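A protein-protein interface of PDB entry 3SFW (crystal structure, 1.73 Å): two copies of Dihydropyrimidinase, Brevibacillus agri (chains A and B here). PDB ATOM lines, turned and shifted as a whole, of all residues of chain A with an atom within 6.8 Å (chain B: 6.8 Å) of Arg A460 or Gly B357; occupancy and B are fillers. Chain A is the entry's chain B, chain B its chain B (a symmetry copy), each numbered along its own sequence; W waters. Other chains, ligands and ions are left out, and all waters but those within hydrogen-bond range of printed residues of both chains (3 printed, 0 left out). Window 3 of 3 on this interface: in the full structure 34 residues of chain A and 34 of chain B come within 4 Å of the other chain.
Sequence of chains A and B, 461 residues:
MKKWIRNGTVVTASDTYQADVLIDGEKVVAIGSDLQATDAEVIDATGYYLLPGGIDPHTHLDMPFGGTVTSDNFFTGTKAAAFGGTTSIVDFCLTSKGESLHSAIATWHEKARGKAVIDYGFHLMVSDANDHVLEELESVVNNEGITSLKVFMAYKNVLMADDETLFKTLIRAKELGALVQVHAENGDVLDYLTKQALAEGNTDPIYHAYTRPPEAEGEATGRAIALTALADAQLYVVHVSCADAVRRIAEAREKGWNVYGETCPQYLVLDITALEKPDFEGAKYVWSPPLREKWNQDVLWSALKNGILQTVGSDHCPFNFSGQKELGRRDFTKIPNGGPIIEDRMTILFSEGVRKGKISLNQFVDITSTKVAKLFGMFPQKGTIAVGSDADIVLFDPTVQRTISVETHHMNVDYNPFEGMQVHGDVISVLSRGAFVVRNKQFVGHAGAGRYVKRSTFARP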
ATOM      1  N   LYS A 174      10.641  -0.318  13.258  1.00  0.00           N
ATOM      2  CA  LYS A 174      11.491   0.365  12.281  1.00  0.00           C
ATOM      3  C   LYS A 174      12.822   0.761  12.955  1.00  0.00           C
ATOM      4  O   LYS A 174      13.916   0.581  12.376  1.00  0.00           O
ATOM      5  CB  LYS A 174      10.821   1.617  11.700  1.00  0.00           C
ATOM      6  CG  LYS A 174      11.709   2.261  10.578  1.00  0.00           C
ATOM      7  CD  LYS A 174      11.401   3.733  10.377  1.00  0.00           C
ATOM      8  CE  LYS A 174      12.229   4.353   9.216  1.00  0.00           C
ATOM      9  NZ  LYS A 174      12.451   3.396   8.052  1.00  0.00           N
ATOM     10  N   GLN A 234       8.146  -1.650   7.843  1.00  0.00           N
ATOM     11  CA  GLN A 234       7.974  -2.761   6.902  1.00  0.00           C
ATOM     12  C   GLN A 234       6.956  -3.773   7.438  1.00  0.00           C
ATOM     13  O   GLN A 234       6.979  -4.126   8.615  1.00  0.00           O
ATOM     14  CB  GLN A 234       9.323  -3.457   6.570  1.00  0.00           C
ATOM     15  CG  GLN A 234      10.254  -3.783   7.765  1.00  0.00           C
ATOM     16  CD  GLN A 234      11.221  -2.620   8.124  1.00  0.00           C
ATOM     17  OE1 GLN A 234      11.463  -1.706   7.310  1.00  0.00           O
ATOM     18  NE2 GLN A 234      11.751  -2.641   9.354  1.00  0.00           N
ATOM     19  N   GLY A 256       5.559   2.137  -3.589  1.00  0.00           N
ATOM     20  CA  GLY A 256       6.921   1.897  -3.135  1.00  0.00           C
ATOM     21  C   GLY A 256       7.026   1.548  -1.655  1.00  0.00           C
ATOM     22  O   GLY A 256       8.137   1.468  -1.119  1.00  0.00           O
ATOM     23  N   ASN A 258       7.043  -0.672   1.798  1.00  0.00           N
ATOM     24  CA  ASN A 258       7.692  -1.953   2.028  1.00  0.00           C
ATOM     25  C   ASN A 258       6.710  -2.931   2.670  1.00  0.00           C
ATOM     26  O   ASN A 258       6.671  -3.109   3.891  1.00  0.00           O
ATOM     27  CB  ASN A 258       8.959  -1.751   2.852  1.00  0.00           C
ATOM     28  CG  ASN A 258       9.961  -0.860   2.119  1.00  0.00           C
ATOM     29  OD1 ASN A 258      10.181  -1.037   0.898  1.00  0.00           O
ATOM     30  ND2 ASN A 258      10.384   0.214   2.773  1.00  0.00           N
ATOM     31  N   TYR A 260       4.904  -6.649   2.200  1.00  0.00           N
ATOM     32  CA  TYR A 260       5.043  -7.986   1.656  1.00  0.00           C
ATOM     33  C   TYR A 260       3.834  -8.816   2.027  1.00  0.00           C
ATOM     34  O   TYR A 260       3.173  -8.553   3.030  1.00  0.00           O
ATOM     35  CB  TYR A 260       6.310  -8.659   2.216  1.00  0.00           C
ATOM     36  CG  TYR A 260       7.516  -7.758   2.021  1.00  0.00           C
ATOM     37  CD1 TYR A 260       7.939  -6.915   3.047  1.00  0.00           C
ATOM     38  CD2 TYR A 260       8.209  -7.743   0.806  1.00  0.00           C
ATOM     39  CE1 TYR A 260       9.001  -6.043   2.855  1.00  0.00           C
ATOM     40  CE2 TYR A 260       9.282  -6.859   0.610  1.00  0.00           C
ATOM     41  CZ  TYR A 260       9.641  -6.014   1.639  1.00  0.00           C
ATOM     42  OH  TYR A 260      10.683  -5.135   1.480  1.00  0.00           O
ATOM     43  N   LYS A 374      15.208 -14.621   3.055  1.00  0.00           N
ATOM     44  CA  LYS A 374      15.598 -13.209   2.934  1.00  0.00           C
ATOM     45  C   LYS A 374      14.725 -12.297   3.797  1.00  0.00           C
ATOM     46  O   LYS A 374      15.236 -11.423   4.478  1.00  0.00           O
ATOM     47  CB  LYS A 374      15.566 -12.771   1.473  1.00  0.00           C
ATOM     48  CG  LYS A 374      16.701 -13.465   0.658  1.00  0.00           C
ATOM     49  CD  LYS A 374      16.654 -13.141  -0.797  1.00  0.00           C
ATOM     50  CE  LYS A 374      18.042 -13.418  -1.419  1.00  0.00           C
ATOM     51  NZ  LYS A 374      17.973 -13.403  -2.891  1.00  0.00           N
ATOM     52  N   LEU A 375      13.412 -12.528   3.805  1.00  0.00           N
ATOM     53  CA  LEU A 375      12.518 -11.680   4.606  1.00  0.00           C
ATOM     54  C   LEU A 375      12.642 -11.913   6.124  1.00  0.00           C
ATOM     55  O   LEU A 375      12.423 -11.010   6.904  1.00  0.00           O
ATOM     56  CB  LEU A 375      11.042 -11.865   4.143  1.00  0.00           C
ATOM     57  CG  LEU A 375      10.718 -11.216   2.782  1.00  0.00           C
ATOM     58  CD1 LEU A 375       9.303 -11.657   2.353  1.00  0.00           C
ATOM     59  CD2 LEU A 375      10.822  -9.685   2.866  1.00  0.00           C
ATOM     60  N   PHE A 458      16.215  -6.722   9.702  1.00  0.00           N
ATOM     61  CA  PHE A 458      15.558  -6.746   8.420  1.00  0.00           C
ATOM     62  C   PHE A 458      16.368  -6.031   7.341  1.00  0.00           C
ATOM     63  O   PHE A 458      16.916  -4.958   7.571  1.00  0.00           O
ATOM     64  CB  PHE A 458      14.166  -6.121   8.530  1.00  0.00           C
ATOM     65  CG  PHE A 458      13.396  -6.180   7.248  1.00  0.00           C
ATOM     66  CD1 PHE A 458      12.797  -7.363   6.841  1.00  0.00           C
ATOM     67  CD2 PHE A 458      13.279  -5.058   6.454  1.00  0.00           C
ATOM     68  CE1 PHE A 458      12.144  -7.439   5.634  1.00  0.00           C
ATOM     69  CE2 PHE A 458      12.570  -5.115   5.272  1.00  0.00           C
ATOM     70  CZ  PHE A 458      12.034  -6.311   4.851  1.00  0.00           C
ATOM     71  N   ALA A 459      16.467  -6.665   6.183  1.00  0.00           N
ATOM     72  CA  ALA A 459      17.012  -6.032   4.973  1.00  0.00           C
ATOM     73  C   ALA A 459      16.107  -6.348   3.789  1.00  0.00           C
ATOM     74  O   ALA A 459      15.636  -7.472   3.648  1.00  0.00           O
ATOM     75  CB  ALA A 459      18.436  -6.539   4.694  1.00  0.00           C
ATOM     76  N   ARG A 460      15.851  -5.359   2.933  1.00  0.00           N
ATOM     77  CA  ARG A 460      14.925  -5.621   1.838  1.00  0.00           C
ATOM     78  C   ARG A 460      15.555  -6.621   0.870  1.00  0.00           C
ATOM     79  O   ARG A 460      16.768  -6.552   0.603  1.00  0.00           O
ATOM     80  CB  ARG A 460      14.537  -4.318   1.130  1.00  0.00           C
ATOM     81  CG  ARG A 460      13.619  -3.436   1.953  1.00  0.00           C
ATOM     82  CD  ARG A 460      13.168  -2.210   1.170  1.00  0.00           C
ATOM     83  NE  ARG A 460      14.284  -1.305   0.886  1.00  0.00           N
ATOM     84  CZ  ARG A 460      14.601  -0.251   1.631  1.00  0.00           C
ATOM     85  NH1 ARG A 460      13.881   0.054   2.725  1.00  0.00           N
ATOM     86  NH2 ARG A 460      15.623   0.517   1.275  1.00  0.00           N
ATOM     87  N   PRO A 461      14.743  -7.547   0.334  1.00  0.00           N
ATOM     88  CA  PRO A 461      15.306  -8.585  -0.530  1.00  0.00           C
ATOM     89  C   PRO A 461      15.717  -8.064  -1.920  1.00  0.00           C
ATOM     90  O   PRO A 461      16.746  -8.583  -2.459  1.00  0.00           O
ATOM     91  CB  PRO A 461      14.183  -9.646  -0.610  1.00  0.00           C
ATOM     92  CG  PRO A 461      12.902  -8.847  -0.271  1.00  0.00           C
ATOM     93  CD  PRO A 461      13.366  -7.858   0.758  1.00  0.00           C
ATOM     94  N   LYS B 305      12.012  -1.911  -7.456  1.00  0.00           N
ATOM     95  CA  LYS B 305      12.161  -2.500  -6.110  1.00  0.00           C
ATOM     96  C   LYS B 305      11.073  -3.517  -5.856  1.00  0.00           C
ATOM     97  O   LYS B 305      11.332  -4.609  -5.322  1.00  0.00           O
ATOM     98  CB  LYS B 305      12.098  -1.417  -5.036  1.00  0.00           C
ATOM     99  CG  LYS B 305      12.095  -1.986  -3.605  1.00  0.00           C
ATOM    100  CD  LYS B 305      12.137  -0.918  -2.538  1.00  0.00           C
ATOM    101  CE  LYS B 305      10.818  -0.179  -2.405  1.00  0.00           C
ATOM    102  NZ  LYS B 305      10.853   0.788  -1.236  1.00  0.00           N
ATOM    103  N   ASN B 306       9.841  -3.158  -6.229  1.00  0.00           N
ATOM    104  CA  ASN B 306       8.690  -4.026  -5.926  1.00  0.00           C
ATOM    105  C   ASN B 306       8.220  -4.928  -7.078  1.00  0.00           C
ATOM    106  O   ASN B 306       7.172  -5.567  -7.004  1.00  0.00           O
ATOM    107  CB  ASN B 306       7.547  -3.182  -5.301  1.00  0.00           C
ATOM    108  CG  ASN B 306       7.788  -2.868  -3.837  1.00  0.00           C
ATOM    109  OD1 ASN B 306       8.577  -3.551  -3.176  1.00  0.00           O
ATOM    110  ND2 ASN B 306       7.137  -1.807  -3.316  1.00  0.00           N
ATOM    111  N   SER B 351      25.233   2.409  -8.489  1.00  0.00           N
ATOM    112  CA  SER B 351      25.582   3.563  -7.658  1.00  0.00           C
ATOM    113  C   SER B 351      24.368   4.371  -7.177  1.00  0.00           C
ATOM    114  O   SER B 351      24.318   4.808  -6.023  1.00  0.00           O
ATOM    115  CB  SER B 351      26.618   4.455  -8.362  1.00  0.00           C
ATOM    116  OG  SER B 351      27.056   5.508  -7.506  1.00  0.00           O
ATOM    117  N   GLU B 352      23.374   4.533  -8.037  1.00  0.00           N
ATOM    118  CA  GLU B 352      22.193   5.298  -7.648  1.00  0.00           C
ATOM    119  C   GLU B 352      21.108   4.355  -7.141  1.00  0.00           C
ATOM    120  O   GLU B 352      20.165   4.792  -6.487  1.00  0.00           O
ATOM    121  CB  GLU B 352      21.655   6.089  -8.825  1.00  0.00           C
ATOM    122  CG  GLU B 352      22.507   7.291  -9.168  1.00  0.00           C
ATOM    123  CD  GLU B 352      22.506   8.323  -8.076  1.00  0.00           C
ATOM    124  OE1 GLU B 352      21.411   8.683  -7.604  1.00  0.00           O
ATOM    125  OE2 GLU B 352      23.591   8.641  -7.567  1.00  0.00           O
ATOM    126  N   GLY B 353      21.220   3.073  -7.473  1.00  0.00           N
ATOM    127  CA  GLY B 353      20.199   2.114  -7.011  1.00  0.00           C
ATOM    128  C   GLY B 353      20.624   1.355  -5.775  1.00  0.00           C
ATOM    129  O   GLY B 353      20.058   1.527  -4.703  1.00  0.00           O
ATOM    130  N   VAL B 354      21.601   0.469  -5.944  1.00  0.00           N
ATOM    131  CA  VAL B 354      22.037  -0.369  -4.833  1.00  0.00           C
ATOM    132  C   VAL B 354      22.553   0.416  -3.650  1.00  0.00           C
ATOM    133  O   VAL B 354      22.123   0.174  -2.508  1.00  0.00           O
ATOM    134  CB  VAL B 354      23.066  -1.445  -5.273  1.00  0.00           C
ATOM    135  CG1 VAL B 354      23.460  -2.329  -4.067  1.00  0.00           C
ATOM    136  CG2 VAL B 354      22.465  -2.297  -6.374  1.00  0.00           C
ATOM    137  N   ARG B 355      23.478   1.343  -3.911  1.00  0.00           N
ATOM    138  CA  ARG B 355      24.165   2.038  -2.849  1.00  0.00           C
ATOM    139  C   ARG B 355      23.234   2.940  -2.062  1.00  0.00           C
ATOM    140  O   ARG B 355      23.485   3.214  -0.877  1.00  0.00           O
ATOM    141  CB  ARG B 355      25.326   2.868  -3.423  1.00  0.00           C
ATOM    142  CG  ARG B 355      26.575   2.081  -3.704  1.00  0.00           C
ATOM    143  CD  ARG B 355      27.754   3.067  -3.893  1.00  0.00           C
ATOM    144  NE  ARG B 355      28.614   3.169  -2.713  1.00  0.00           N
ATOM    145  CZ  ARG B 355      28.785   4.266  -1.982  1.00  0.00           C
ATOM    146  NH1 ARG B 355      28.121   5.386  -2.253  1.00  0.00           N
ATOM    147  NH2 ARG B 355      29.596   4.227  -0.941  1.00  0.00           N
ATOM    148  N   LYS B 356      22.158   3.391  -2.708  1.00  0.00           N
ATOM    149  CA  LYS B 356      21.165   4.237  -2.076  1.00  0.00           C
ATOM    150  C   LYS B 356      19.940   3.489  -1.526  1.00  0.00           C
ATOM    151  O   LYS B 356      18.974   4.115  -1.079  1.00  0.00           O
ATOM    152  CB  LYS B 356      20.712   5.320  -3.049  1.00  0.00           C
ATOM    153  CG  LYS B 356      21.871   6.201  -3.552  1.00  0.00           C
ATOM    154  CD  LYS B 356      21.345   7.541  -4.047  1.00  0.00           C
ATOM    155  CE  LYS B 356      22.478   8.545  -4.324  1.00  0.00           C
ATOM    156  NZ  LYS B 356      21.890   9.796  -4.961  1.00  0.00           N
ATOM    157  N   GLY B 357      19.967   2.158  -1.558  1.00  0.00           N
ATOM    158  CA  GLY B 357      18.902   1.382  -0.937  1.00  0.00           C
ATOM    159  C   GLY B 357      17.619   1.326  -1.759  1.00  0.00           C
ATOM    160  O   GLY B 357      16.594   0.891  -1.259  1.00  0.00           O
ATOM    161  N   LYS B 358      17.671   1.749  -3.023  1.00  0.00           N
ATOM    162  CA  LYS B 358      16.469   1.730  -3.881  1.00  0.00           C
ATOM    163  C   LYS B 358      16.154   0.347  -4.384  1.00  0.00           C
ATOM    164  O   LYS B 358      15.003   0.053  -4.657  1.00  0.00           O
ATOM    165  CB  LYS B 358      16.589   2.701  -5.041  1.00  0.00           C
ATOM    166  CG  LYS B 358      16.971   4.064  -4.531  1.00  0.00           C
ATOM    167  CD  LYS B 358      16.578   5.188  -5.408  1.00  0.00           C
ATOM    168  CE  LYS B 358      16.834   6.509  -4.656  1.00  0.00           C
ATOM    169  NZ  LYS B 358      16.765   7.726  -5.535  1.00  0.00           N
ATOM    170  N   ILE B 359      17.197  -0.445  -4.636  1.00  0.00           N
ATOM    171  CA  ILE B 359      17.049  -1.841  -5.012  1.00  0.00           C
ATOM    172  C   ILE B 359      18.128  -2.616  -4.280  1.00  0.00           C
ATOM    173  O   ILE B 359      19.123  -2.028  -3.858  1.00  0.00           O
ATOM    174  CB  ILE B 359      17.246  -2.055  -6.544  1.00  0.00           C
ATOM    175  CG1 ILE B 359      18.507  -1.321  -7.051  1.00  0.00           C
ATOM    176  CG2 ILE B 359      16.009  -1.570  -7.340  1.00  0.00           C
ATOM    177  CD1 ILE B 359      18.872  -1.673  -8.501  1.00  0.00           C
ATOM    178  N   SER B 360      17.956  -3.924  -4.129  1.00  0.00           N
ATOM    179  CA  SER B 360      19.035  -4.706  -3.528  1.00  0.00           C
ATOM    180  C   SER B 360      20.129  -5.051  -4.545  1.00  0.00           C
ATOM    181  O   SER B 360      19.914  -4.995  -5.751  1.00  0.00           O
ATOM    182  CB  SER B 360      18.512  -5.959  -2.860  1.00  0.00           C
ATOM    183  OG  SER B 360      18.202  -6.940  -3.821  1.00  0.00           O
ATOM    184  N   LEU B 361      21.295  -5.447  -4.038  1.00  0.00           N
ATOM    185  CA  LEU B 361      22.341  -6.012  -4.886  1.00  0.00           C
ATOM    186  C   LEU B 361      21.896  -7.178  -5.774  1.00  0.00           C
ATOM    187  O   LEU B 361      22.240  -7.213  -6.944  1.00  0.00           O
ATOM    188  CB  LEU B 361      23.546  -6.408  -4.020  1.00  0.00           C
ATOM    189  CG  LEU B 361      24.849  -6.818  -4.684  1.00  0.00           C
ATOM    190  CD1 LEU B 361      25.415  -5.646  -5.485  1.00  0.00           C
ATOM    191  CD2 LEU B 361      25.799  -7.206  -3.504  1.00  0.00           C
ATOM    192  N   GLN B 363      18.773  -7.816  -6.725  1.00  0.00           N
ATOM    193  CA  GLN B 363      17.852  -7.250  -7.718  1.00  0.00           C
ATOM    194  C   GLN B 363      18.581  -6.548  -8.835  1.00  0.00           C
ATOM    195  O   GLN B 363      18.124  -6.558  -9.963  1.00  0.00           O
ATOM    196  CB  GLN B 363      16.877  -6.253  -7.077  1.00  0.00           C
ATOM    197  CG  GLN B 363      15.892  -6.903  -6.137  1.00  0.00           C
ATOM    198  CD  GLN B 363      14.925  -5.878  -5.564  1.00  0.00           C
ATOM    199  OE1 GLN B 363      15.348  -4.839  -5.064  1.00  0.00           O
ATOM    200  NE2 GLN B 363      13.608  -6.113  -5.754  1.00  0.00           N
HETATM  201  O   HOH W   1      11.340   2.507   1.090  1.00  0.00           O
HETATM  202  O   HOH W   2       9.981  -3.247  -0.774  1.00  0.00           O
HETATM  203  O   HOH W   3      15.513  -2.138  -1.671  1.00  0.00           O
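O of Pro A461 lies within hydrogen-bond range of OG of Ser B360, at 2.6 Å.
The backbone carbonyl oxygen of Gly A256 lies within hydrogen-bond range of the side-chain amino group of Lys B305.
OD1 of Asn A258 sits at hydrogen-bond distance from NZ of Lys B305 (2.9 Å).
The backbone carbonyl oxygen of Gly B357 is in hydrogen-bond range of the guanidinium group of Arg A460 (2.7 Å).
NE2 of Gln B363 is in hydrogen-bond range of O of Lys B305 (2.8 Å).
The side-chain amide oxygen (OE1) of Gln B363 sits at hydrogen-bond distance from the backbone NH (N) of Ser B360.
Gly A256 touches Asn B306 (CA to ND2, 3.7 Å).
Ser B360 touches Arg A460 (CB to O, 3.9 Å).
Of chain B, only Gly B357 and Ser B360 come within 4 Å of Arg A460.
Of chain A, only Arg A460 comes within 4 Å of Gly B357.
Printed residues of chain A within 4 Å of Asn B306: Gly A256 (3.7 Å).
Printed residues of chain A within 4 Å of Ser B360: Arg A460 (3.9 Å) and Pro A461 (2.6 Å).
Of the printed residues of chain B, Gly A256 touches Lys B305 and Asn B306.
Printed residues of chain B within 4 Å of Pro A461: Ser B360.
Of the printed residues of chain A, Lys B305 touches Gly A256 (2.8 Å) and Asn A258 (2.9 Å).
Gly B353 touches none of the printed residues of chain A.
Of the 14 printed residues of chain B, 4 touch a printed residue of chain A.
Printed residues of chain B that touch a printed residue of chain A: Lys B305, Asn B306, Gly B357 and Ser B360.
Along chain B the printed residues that touch a printed residue of chain A span positions 305 to 360.
Of the 11 printed residues of chain A, 4 touch a printed residue of chain B.
Among the printed residues, 6 pairs touch across the chains.
Among the printed residues, no Asp or Glu carboxylate lies within 4 Å of a Lys or Arg side-chain nitrogen of the other chain.
No position is printed for both chains.
Of the 6 pairs that touch across the chains among the printed residues, none has its exchanged pair printed and touching as well.
Water W2 lies within hydrogen-bond range of OD1 of Asn A258 (2.8 Å), OD1 of Asn B306 (2.8 Å) and OH of Tyr A260 (3.0 Å).
Water W1 lies within hydrogen-bond range of the side-chain amino group (NZ) of Lys B305 (2.9 Å) and the side-chain amide nitrogen (ND2) of Asn A258 (3.0 Å).
Water W3 bridges the guanidinium group (NE) of Arg A460 (3.0 Å) and the backbone carbonyl oxygen (O) of Gly B357 (3.2 Å).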
